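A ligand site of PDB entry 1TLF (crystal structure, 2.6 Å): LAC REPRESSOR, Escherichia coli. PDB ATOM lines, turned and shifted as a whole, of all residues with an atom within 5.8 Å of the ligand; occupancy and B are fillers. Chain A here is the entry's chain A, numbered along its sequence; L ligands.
The side-chain carboxylate (OD2) of Asp 215 lies within hydrogen-bond range of an oxygen (O2) of the ligand (2.6 Å). The guanidinium group (NH2) of Arg 138 lies within hydrogen-bond range of an oxygen (O1) of the ligand (2.8 Å). The side-chain amide nitrogen of Asn 187 sits at hydrogen-bond distance from an oxygen (O2) of the ligand (2.8 Å). The side-chain carboxylate (OD2) of Asp 90 lies within hydrogen-bond range of an oxygen (O5) of the ligand, at 3.2 Å.
OD1 of Asp 215 sits close to OE1 of Gln 232 (3.0 Å). The guanidinium group (NH2) of Arg 138 sits at hydrogen-bond distance from the side-chain amide oxygen (OE1) of Gln 232 (3.3 Å). The guanidinium group (NH1) of Arg 138 sits at hydrogen-bond distance from the backbone carbonyl oxygen (O) of Ala 186, at 2.5 Å. The side-chain amide nitrogen of Asn 187 sits close to the backbone carbonyl oxygen of Trp 161, 3.0 Å away. N of Gln 189 sits at hydrogen-bond distance from OD1 of Asn 187 (3.3 Å). The side-chain hydroxyl (OG) of Ser 134 is in hydrogen-bond range of the side-chain carboxylate (OD1) of Asp 90 (2.7 Å). The backbone carbonyl oxygen (O) of Asn 66 lies within hydrogen-bond range of the side-chain hydroxyl (OG) of Ser 10, at 3.5 Å.
Merely in contact with the ligand: Ser 134 (3.2 Å), Ala 16 (3.2 Å), Pro 17 (3.3 Å), Leu 89 (3.5 Å), Trp 161 (3.6 Å), Gln 232 (3.7 Å), Leu 14 (3.9 Å), Ile 20 (3.9 Å), Pro 68 (3.9 Å) and Ser 10 (3.998 Å). Hydrophobic or aromatic side chains that line the ligand: Leu 14, Ala 16, Pro 17, Ile 20, Pro 68 and Trp 161. 14 residues have an atom within 4 Å of the ligand: Ser 10, Leu 14, Ala 16, Pro 17, Ile 20, Pro 68, Leu 89, Asp 90, Ser 134, Arg 138, Trp 161, Asn 187, Asp 215 and Gln 232. The nearest printed residue that does not touch the ligand is Asn 66 (4.01 Å).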
ATOM      1  N   SER A  10      -3.343  19.048 -21.077  1.00  0.00           N
ATOM      2  CA  SER A  10      -3.681  19.126 -19.669  1.00  0.00           C
ATOM      3  C   SER A  10      -2.492  18.422 -18.987  1.00  0.00           C
ATOM      4  O   SER A  10      -1.565  17.976 -19.679  1.00  0.00           O
ATOM      5  CB  SER A  10      -5.019  18.436 -19.364  1.00  0.00           C
ATOM      6  OG  SER A  10      -5.137  17.147 -19.931  1.00  0.00           O
ATOM      7  N   LEU A  14      -0.776  12.824 -15.632  1.00  0.00           N
ATOM      8  CA  LEU A  14      -1.684  11.706 -15.877  1.00  0.00           C
ATOM      9  C   LEU A  14      -1.115  10.972 -17.098  1.00  0.00           C
ATOM     10  O   LEU A  14      -0.532  11.612 -17.980  1.00  0.00           O
ATOM     11  CB  LEU A  14      -3.104  12.236 -16.104  1.00  0.00           C
ATOM     12  CG  LEU A  14      -3.714  13.143 -15.025  1.00  0.00           C
ATOM     13  CD1 LEU A  14      -5.000  13.681 -15.526  1.00  0.00           C
ATOM     14  CD2 LEU A  14      -3.953  12.429 -13.746  1.00  0.00           C
ATOM     15  N   HIS A  15      -1.262   9.652 -17.179  1.00  0.00           N
ATOM     16  CA  HIS A  15      -0.686   8.901 -18.300  1.00  0.00           C
ATOM     17  C   HIS A  15      -1.347   9.059 -19.674  1.00  0.00           C
ATOM     18  O   HIS A  15      -0.665   9.157 -20.691  1.00  0.00           O
ATOM     19  CB  HIS A  15      -0.536   7.416 -17.930  1.00  0.00           C
ATOM     20  CG  HIS A  15      -0.016   7.188 -16.549  1.00  0.00           C
ATOM     21  ND1 HIS A  15       0.592   8.184 -15.808  1.00  0.00           N
ATOM     22  CD2 HIS A  15      -0.105   6.112 -15.730  1.00  0.00           C
ATOM     23  CE1 HIS A  15       0.863   7.727 -14.603  1.00  0.00           C
ATOM     24  NE2 HIS A  15       0.448   6.477 -14.522  1.00  0.00           N
ATOM     25  N   ALA A  16      -2.665   9.085 -19.713  1.00  0.00           N
ATOM     26  CA  ALA A  16      -3.342   9.227 -20.983  1.00  0.00           C
ATOM     27  C   ALA A  16      -2.792  10.433 -21.731  1.00  0.00           C
ATOM     28  O   ALA A  16      -2.299  10.312 -22.854  1.00  0.00           O
ATOM     29  CB  ALA A  16      -4.806   9.318 -20.779  1.00  0.00           C
ATOM     30  N   PRO A  17      -2.802  11.615 -21.081  1.00  0.00           N
ATOM     31  CA  PRO A  17      -2.273  12.797 -21.762  1.00  0.00           C
ATOM     32  C   PRO A  17      -0.825  12.618 -22.256  1.00  0.00           C
ATOM     33  O   PRO A  17      -0.537  12.790 -23.453  1.00  0.00           O
ATOM     34  CB  PRO A  17      -2.402  13.848 -20.681  1.00  0.00           C
ATOM     35  CG  PRO A  17      -3.688  13.495 -20.080  1.00  0.00           C
ATOM     36  CD  PRO A  17      -3.512  12.028 -19.863  1.00  0.00           C
ATOM     37  N   ILE A  20      -0.873  10.556 -25.213  1.00  0.00           N
ATOM     38  CA  ILE A  20      -1.402  11.164 -26.413  1.00  0.00           C
ATOM     39  C   ILE A  20      -0.344  12.009 -27.027  1.00  0.00           C
ATOM     40  O   ILE A  20       0.011  11.803 -28.215  1.00  0.00           O
ATOM     41  CB  ILE A  20      -2.656  11.958 -26.149  1.00  0.00           C
ATOM     42  CG1 ILE A  20      -3.762  10.998 -25.695  1.00  0.00           C
ATOM     43  CG2 ILE A  20      -3.046  12.712 -27.437  1.00  0.00           C
ATOM     44  CD1 ILE A  20      -4.843  11.623 -24.939  1.00  0.00           C
ATOM     45  N   ASN A  66      -5.705  19.178 -26.329  1.00  0.00           N
ATOM     46  CA  ASN A  66      -6.013  17.955 -25.606  1.00  0.00           C
ATOM     47  C   ASN A  66      -6.456  18.241 -24.171  1.00  0.00           C
ATOM     48  O   ASN A  66      -6.155  17.489 -23.245  1.00  0.00           O
ATOM     49  CB  ASN A  66      -4.796  17.050 -25.681  1.00  0.00           C
ATOM     50  CG  ASN A  66      -5.003  15.749 -24.963  1.00  0.00           C
ATOM     51  OD1 ASN A  66      -4.048  15.157 -24.462  1.00  0.00           O
ATOM     52  ND2 ASN A  66      -6.247  15.299 -24.891  1.00  0.00           N
ATOM     53  N   PRO A  68      -9.899  19.382 -21.523  1.00  0.00           N
ATOM     54  CA  PRO A  68     -11.329  19.273 -21.230  1.00  0.00           C
ATOM     55  C   PRO A  68     -12.109  20.597 -21.316  1.00  0.00           C
ATOM     56  O   PRO A  68     -11.823  21.559 -20.580  1.00  0.00           O
ATOM     57  CB  PRO A  68     -11.340  18.780 -19.785  1.00  0.00           C
ATOM     58  CG  PRO A  68     -10.068  18.000 -19.692  1.00  0.00           C
ATOM     59  CD  PRO A  68      -9.100  18.879 -20.396  1.00  0.00           C
ATOM     60  N   LEU A  89      -9.472  17.267 -28.704  1.00  0.00           N
ATOM     61  CA  LEU A  89      -9.496  15.841 -28.414  1.00  0.00           C
ATOM     62  C   LEU A  89     -10.239  15.478 -27.142  1.00  0.00           C
ATOM     63  O   LEU A  89     -10.475  14.302 -26.886  1.00  0.00           O
ATOM     64  CB  LEU A  89      -8.087  15.278 -28.275  1.00  0.00           C
ATOM     65  CG  LEU A  89      -7.063  15.595 -29.359  1.00  0.00           C
ATOM     66  CD1 LEU A  89      -5.811  14.795 -29.091  1.00  0.00           C
ATOM     67  CD2 LEU A  89      -7.583  15.247 -30.698  1.00  0.00           C
ATOM     68  N   ASP A  90     -10.583  16.463 -26.322  1.00  0.00           N
ATOM     69  CA  ASP A  90     -11.267  16.198 -25.061  1.00  0.00           C
ATOM     70  C   ASP A  90     -12.581  16.978 -24.972  1.00  0.00           C
ATOM     71  O   ASP A  90     -12.798  17.765 -24.050  1.00  0.00           O
ATOM     72  CB  ASP A  90     -10.348  16.567 -23.904  1.00  0.00           C
ATOM     73  CG  ASP A  90     -10.586  15.736 -22.682  1.00  0.00           C
ATOM     74  OD1 ASP A  90     -11.751  15.386 -22.399  1.00  0.00           O
ATOM     75  OD2 ASP A  90      -9.584  15.438 -21.981  1.00  0.00           O
ATOM     76  N   PHE A 102     -12.994   9.491 -28.879  1.00  0.00           N
ATOM     77  CA  PHE A 102     -13.302   8.061 -28.930  1.00  0.00           C
ATOM     78  C   PHE A 102     -14.771   7.933 -28.606  1.00  0.00           C
ATOM     79  O   PHE A 102     -15.404   8.905 -28.149  1.00  0.00           O
ATOM     80  CB  PHE A 102     -12.500   7.271 -27.884  1.00  0.00           C
ATOM     81  CG  PHE A 102     -11.049   7.090 -28.209  1.00  0.00           C
ATOM     82  CD1 PHE A 102     -10.643   6.071 -29.047  1.00  0.00           C
ATOM     83  CD2 PHE A 102     -10.085   7.931 -27.664  1.00  0.00           C
ATOM     84  CE1 PHE A 102      -9.310   5.885 -29.323  1.00  0.00           C
ATOM     85  CE2 PHE A 102      -8.751   7.755 -27.940  1.00  0.00           C
ATOM     86  CZ  PHE A 102      -8.361   6.727 -28.766  1.00  0.00           C
ATOM     87  N   SER A 132     -14.830  17.289 -16.116  1.00  0.00           N
ATOM     88  CA  SER A 132     -14.412  16.680 -17.361  1.00  0.00           C
ATOM     89  C   SER A 132     -15.598  16.187 -18.183  1.00  0.00           C
ATOM     90  O   SER A 132     -16.368  15.351 -17.725  1.00  0.00           O
ATOM     91  CB  SER A 132     -13.462  15.519 -17.067  1.00  0.00           C
ATOM     92  OG  SER A 132     -12.807  15.067 -18.241  1.00  0.00           O
ATOM     93  N   SER A 134     -15.482  14.261 -20.678  1.00  0.00           N
ATOM     94  CA  SER A 134     -15.296  12.813 -20.892  1.00  0.00           C
ATOM     95  C   SER A 134     -15.694  12.062 -19.627  1.00  0.00           C
ATOM     96  O   SER A 134     -16.332  11.020 -19.684  1.00  0.00           O
ATOM     97  CB  SER A 134     -13.852  12.524 -21.252  1.00  0.00           C
ATOM     98  OG  SER A 134     -13.440  13.342 -22.335  1.00  0.00           O
ATOM     99  N   ARG A 138     -18.917   9.487 -19.731  1.00  0.00           N
ATOM    100  CA  ARG A 138     -18.776   8.109 -19.312  1.00  0.00           C
ATOM    101  C   ARG A 138     -19.733   7.783 -18.181  1.00  0.00           C
ATOM    102  O   ARG A 138     -20.400   6.743 -18.226  1.00  0.00           O
ATOM    103  CB  ARG A 138     -17.342   7.825 -18.876  1.00  0.00           C
ATOM    104  CG  ARG A 138     -16.316   7.945 -20.015  1.00  0.00           C
ATOM    105  CD  ARG A 138     -14.882   7.817 -19.506  1.00  0.00           C
ATOM    106  NE  ARG A 138     -13.953   8.365 -20.475  1.00  0.00           N
ATOM    107  CZ  ARG A 138     -12.639   8.482 -20.307  1.00  0.00           C
ATOM    108  NH1 ARG A 138     -12.045   8.075 -19.188  1.00  0.00           N
ATOM    109  NH2 ARG A 138     -11.916   9.016 -21.286  1.00  0.00           N
ATOM    110  N   TRP A 161      -8.775  11.354 -11.512  1.00  0.00           N
ATOM    111  CA  TRP A 161      -7.886  10.781 -12.521  1.00  0.00           C
ATOM    112  C   TRP A 161      -6.631  10.115 -12.024  1.00  0.00           C
ATOM    113  O   TRP A 161      -5.956   9.402 -12.787  1.00  0.00           O
ATOM    114  CB  TRP A 161      -7.534  11.797 -13.630  1.00  0.00           C
ATOM    115  CG  TRP A 161      -8.687  12.260 -14.510  1.00  0.00           C
ATOM    116  CD1 TRP A 161      -8.977  13.553 -14.839  1.00  0.00           C
ATOM    117  CD2 TRP A 161      -9.655  11.448 -15.180  1.00  0.00           C
ATOM    118  NE1 TRP A 161     -10.062  13.595 -15.662  1.00  0.00           N
ATOM    119  CE2 TRP A 161     -10.494  12.318 -15.889  1.00  0.00           C
ATOM    120  CE3 TRP A 161      -9.892  10.084 -15.242  1.00  0.00           C
ATOM    121  CZ2 TRP A 161     -11.569  11.853 -16.659  1.00  0.00           C
ATOM    122  CZ3 TRP A 161     -10.939   9.625 -15.995  1.00  0.00           C
ATOM    123  CH2 TRP A 161     -11.763  10.503 -16.703  1.00  0.00           C
ATOM    124  N   ALA A 186     -13.551   5.226 -14.139  1.00  0.00           N
ATOM    125  CA  ALA A 186     -13.324   6.200 -15.240  1.00  0.00           C
ATOM    126  C   ALA A 186     -12.013   6.092 -16.031  1.00  0.00           C
ATOM    127  O   ALA A 186     -11.941   6.510 -17.193  1.00  0.00           O
ATOM    128  CB  ALA A 186     -13.492   7.594 -14.715  1.00  0.00           C
ATOM    129  N   ASN A 187     -10.961   5.582 -15.390  1.00  0.00           N
ATOM    130  CA  ASN A 187      -9.683   5.357 -16.049  1.00  0.00           C
ATOM    131  C   ASN A 187      -8.921   4.326 -15.242  1.00  0.00           C
ATOM    132  O   ASN A 187      -9.362   3.933 -14.156  1.00  0.00           O
ATOM    133  CB  ASN A 187      -8.914   6.668 -16.242  1.00  0.00           C
ATOM    134  CG  ASN A 187      -8.254   7.171 -14.975  1.00  0.00           C
ATOM    135  OD1 ASN A 187      -8.328   6.550 -13.919  1.00  0.00           O
ATOM    136  ND2 ASN A 187      -7.583   8.312 -15.080  1.00  0.00           N
ATOM    137  N   ASP A 188      -7.799   3.863 -15.772  1.00  0.00           N
ATOM    138  CA  ASP A 188      -6.976   2.847 -15.109  1.00  0.00           C
ATOM    139  C   ASP A 188      -6.181   3.322 -13.883  1.00  0.00           C
ATOM    140  O   ASP A 188      -6.067   2.582 -12.913  1.00  0.00           O
ATOM    141  CB  ASP A 188      -6.038   2.171 -16.135  1.00  0.00           C
ATOM    142  CG  ASP A 188      -6.806   1.444 -17.233  1.00  0.00           C
ATOM    143  OD1 ASP A 188      -8.044   1.334 -17.146  1.00  0.00           O
ATOM    144  OD2 ASP A 188      -6.174   0.979 -18.204  1.00  0.00           O
ATOM    145  N   GLN A 189      -5.659   4.539 -13.902  1.00  0.00           N
ATOM    146  CA  GLN A 189      -4.893   5.023 -12.756  1.00  0.00           C
ATOM    147  C   GLN A 189      -5.740   4.913 -11.532  1.00  0.00           C
ATOM    148  O   GLN A 189      -5.311   4.386 -10.525  1.00  0.00           O
ATOM    149  CB  GLN A 189      -4.421   6.455 -12.927  1.00  0.00           C
ATOM    150  CG  GLN A 189      -3.088   6.538 -13.591  1.00  0.00           C
ATOM    151  CD  GLN A 189      -2.739   7.927 -13.995  1.00  0.00           C
ATOM    152  OE1 GLN A 189      -3.204   8.417 -15.028  1.00  0.00           O
ATOM    153  NE2 GLN A 189      -1.899   8.580 -13.209  1.00  0.00           N
ATOM    154  N   TYR A 214     -10.542   2.098 -17.657  1.00  0.00           N
ATOM    155  CA  TYR A 214     -10.710   2.784 -18.933  1.00  0.00           C
ATOM    156  C   TYR A 214      -9.370   3.305 -19.398  1.00  0.00           C
ATOM    157  O   TYR A 214      -8.592   3.768 -18.557  1.00  0.00           O
ATOM    158  CB  TYR A 214     -11.629   3.977 -18.718  1.00  0.00           C
ATOM    159  CG  TYR A 214     -12.648   4.164 -19.804  1.00  0.00           C
ATOM    160  CD1 TYR A 214     -12.366   4.924 -20.928  1.00  0.00           C
ATOM    161  CD2 TYR A 214     -13.939   3.633 -19.677  1.00  0.00           C
ATOM    162  CE1 TYR A 214     -13.321   5.146 -21.879  1.00  0.00           C
ATOM    163  CE2 TYR A 214     -14.885   3.864 -20.634  1.00  0.00           C
ATOM    164  CZ  TYR A 214     -14.571   4.620 -21.720  1.00  0.00           C
ATOM    165  OH  TYR A 214     -15.518   4.860 -22.663  1.00  0.00           O
ATOM    166  N   ASP A 215      -9.096   3.204 -20.712  1.00  0.00           N
ATOM    167  CA  ASP A 215      -7.852   3.667 -21.394  1.00  0.00           C
ATOM    168  C   ASP A 215      -6.855   2.616 -21.857  1.00  0.00           C
ATOM    169  O   ASP A 215      -6.273   2.737 -22.943  1.00  0.00           O
ATOM    170  CB  ASP A 215      -7.004   4.637 -20.545  1.00  0.00           C
ATOM    171  CG  ASP A 215      -7.612   6.011 -20.388  1.00  0.00           C
ATOM    172  OD1 ASP A 215      -8.469   6.407 -21.200  1.00  0.00           O
ATOM    173  OD2 ASP A 215      -7.213   6.708 -19.440  1.00  0.00           O
ATOM    174  N   GLN A 232      -8.441   2.608 -25.420  1.00  0.00           N
ATOM    175  CA  GLN A 232      -8.584   3.766 -26.294  1.00  0.00           C
ATOM    176  C   GLN A 232      -7.236   3.811 -27.016  1.00  0.00           C
ATOM    177  O   GLN A 232      -6.202   3.856 -26.376  1.00  0.00           O
ATOM    178  CB  GLN A 232      -8.792   5.021 -25.461  1.00  0.00           C
ATOM    179  CG  GLN A 232      -9.915   4.936 -24.420  1.00  0.00           C
ATOM    180  CD  GLN A 232     -10.664   6.268 -24.226  1.00  0.00           C
ATOM    181  OE1 GLN A 232     -10.225   7.169 -23.511  1.00  0.00           O
ATOM    182  NE2 GLN A 232     -11.788   6.393 -24.897  1.00  0.00           N
ATOM    183  N   PHE A 234      -4.460   5.477 -28.353  1.00  0.00           N
ATOM    184  CA  PHE A 234      -3.806   6.797 -28.405  1.00  0.00           C
ATOM    185  C   PHE A 234      -2.758   6.962 -29.504  1.00  0.00           C
ATOM    186  O   PHE A 234      -2.203   8.035 -29.650  1.00  0.00           O
ATOM    187  CB  PHE A 234      -3.201   7.147 -27.045  1.00  0.00           C
ATOM    188  CG  PHE A 234      -4.195   7.013 -25.884  1.00  0.00           C
ATOM    189  CD1 PHE A 234      -5.364   7.776 -25.857  1.00  0.00           C
ATOM    190  CD2 PHE A 234      -3.917   6.192 -24.815  1.00  0.00           C
ATOM    191  CE1 PHE A 234      -6.202   7.717 -24.792  1.00  0.00           C
ATOM    192  CE2 PHE A 234      -4.770   6.133 -23.737  1.00  0.00           C
ATOM    193  CZ  PHE A 234      -5.902   6.895 -23.729  1.00  0.00           C
ATOM    194  N   LEU A 237      -5.079   7.888 -32.088  1.00  0.00           N
ATOM    195  CA  LEU A 237      -5.527   9.224 -31.701  1.00  0.00           C
ATOM    196  C   LEU A 237      -4.477  10.300 -32.024  1.00  0.00           C
ATOM    197  O   LEU A 237      -4.830  11.436 -32.346  1.00  0.00           O
ATOM    198  CB  LEU A 237      -5.902   9.260 -30.227  1.00  0.00           C
ATOM    199  CG  LEU A 237      -6.680  10.450 -29.682  1.00  0.00           C
ATOM    200  CD1 LEU A 237      -5.735  11.455 -29.164  1.00  0.00           C
ATOM    201  CD2 LEU A 237      -7.582  11.057 -30.733  1.00  0.00           C
HETATM  202  C1  LIG L   1      -8.682  10.932 -20.683  1.00  0.00           C
HETATM  203  C2  LIG L   1      -8.358   9.629 -19.947  1.00  0.00           C
HETATM  204  O1  LIG L   1      -9.370   8.682 -20.225  1.00  0.00           O
HETATM  205  C3  LIG L   1      -8.255   9.805 -18.415  1.00  0.00           C
HETATM  206  O2  LIG L   1      -7.605   8.688 -17.842  1.00  0.00           O
HETATM  207  C4  LIG L   1      -7.494  11.065 -18.022  1.00  0.00           C
HETATM  208  O3  LIG L   1      -6.113  10.893 -18.259  1.00  0.00           O
HETATM  209  C5  LIG L   1      -8.033  12.229 -18.819  1.00  0.00           C
HETATM  210  O4  LIG L   1      -7.859  11.981 -20.214  1.00  0.00           O
HETATM  211  C6  LIG L   1      -7.399  13.578 -18.543  1.00  0.00           C
HETATM  212  O5  LIG L   1      -8.136  14.607 -19.199  1.00  0.00           O
HETATM  213  S1  LIG L   1      -8.276  10.730 -22.407  1.00  0.00           S
HETATM  214  C7  LIG L   1      -9.010  12.172 -23.235  1.00  0.00           C
HETATM  215  C8  LIG L   1      -8.719  12.142 -24.715  1.00  0.00           C
HETATM  216  C9  LIG L   1     -10.511  12.274 -22.998  1.00  0.00           C
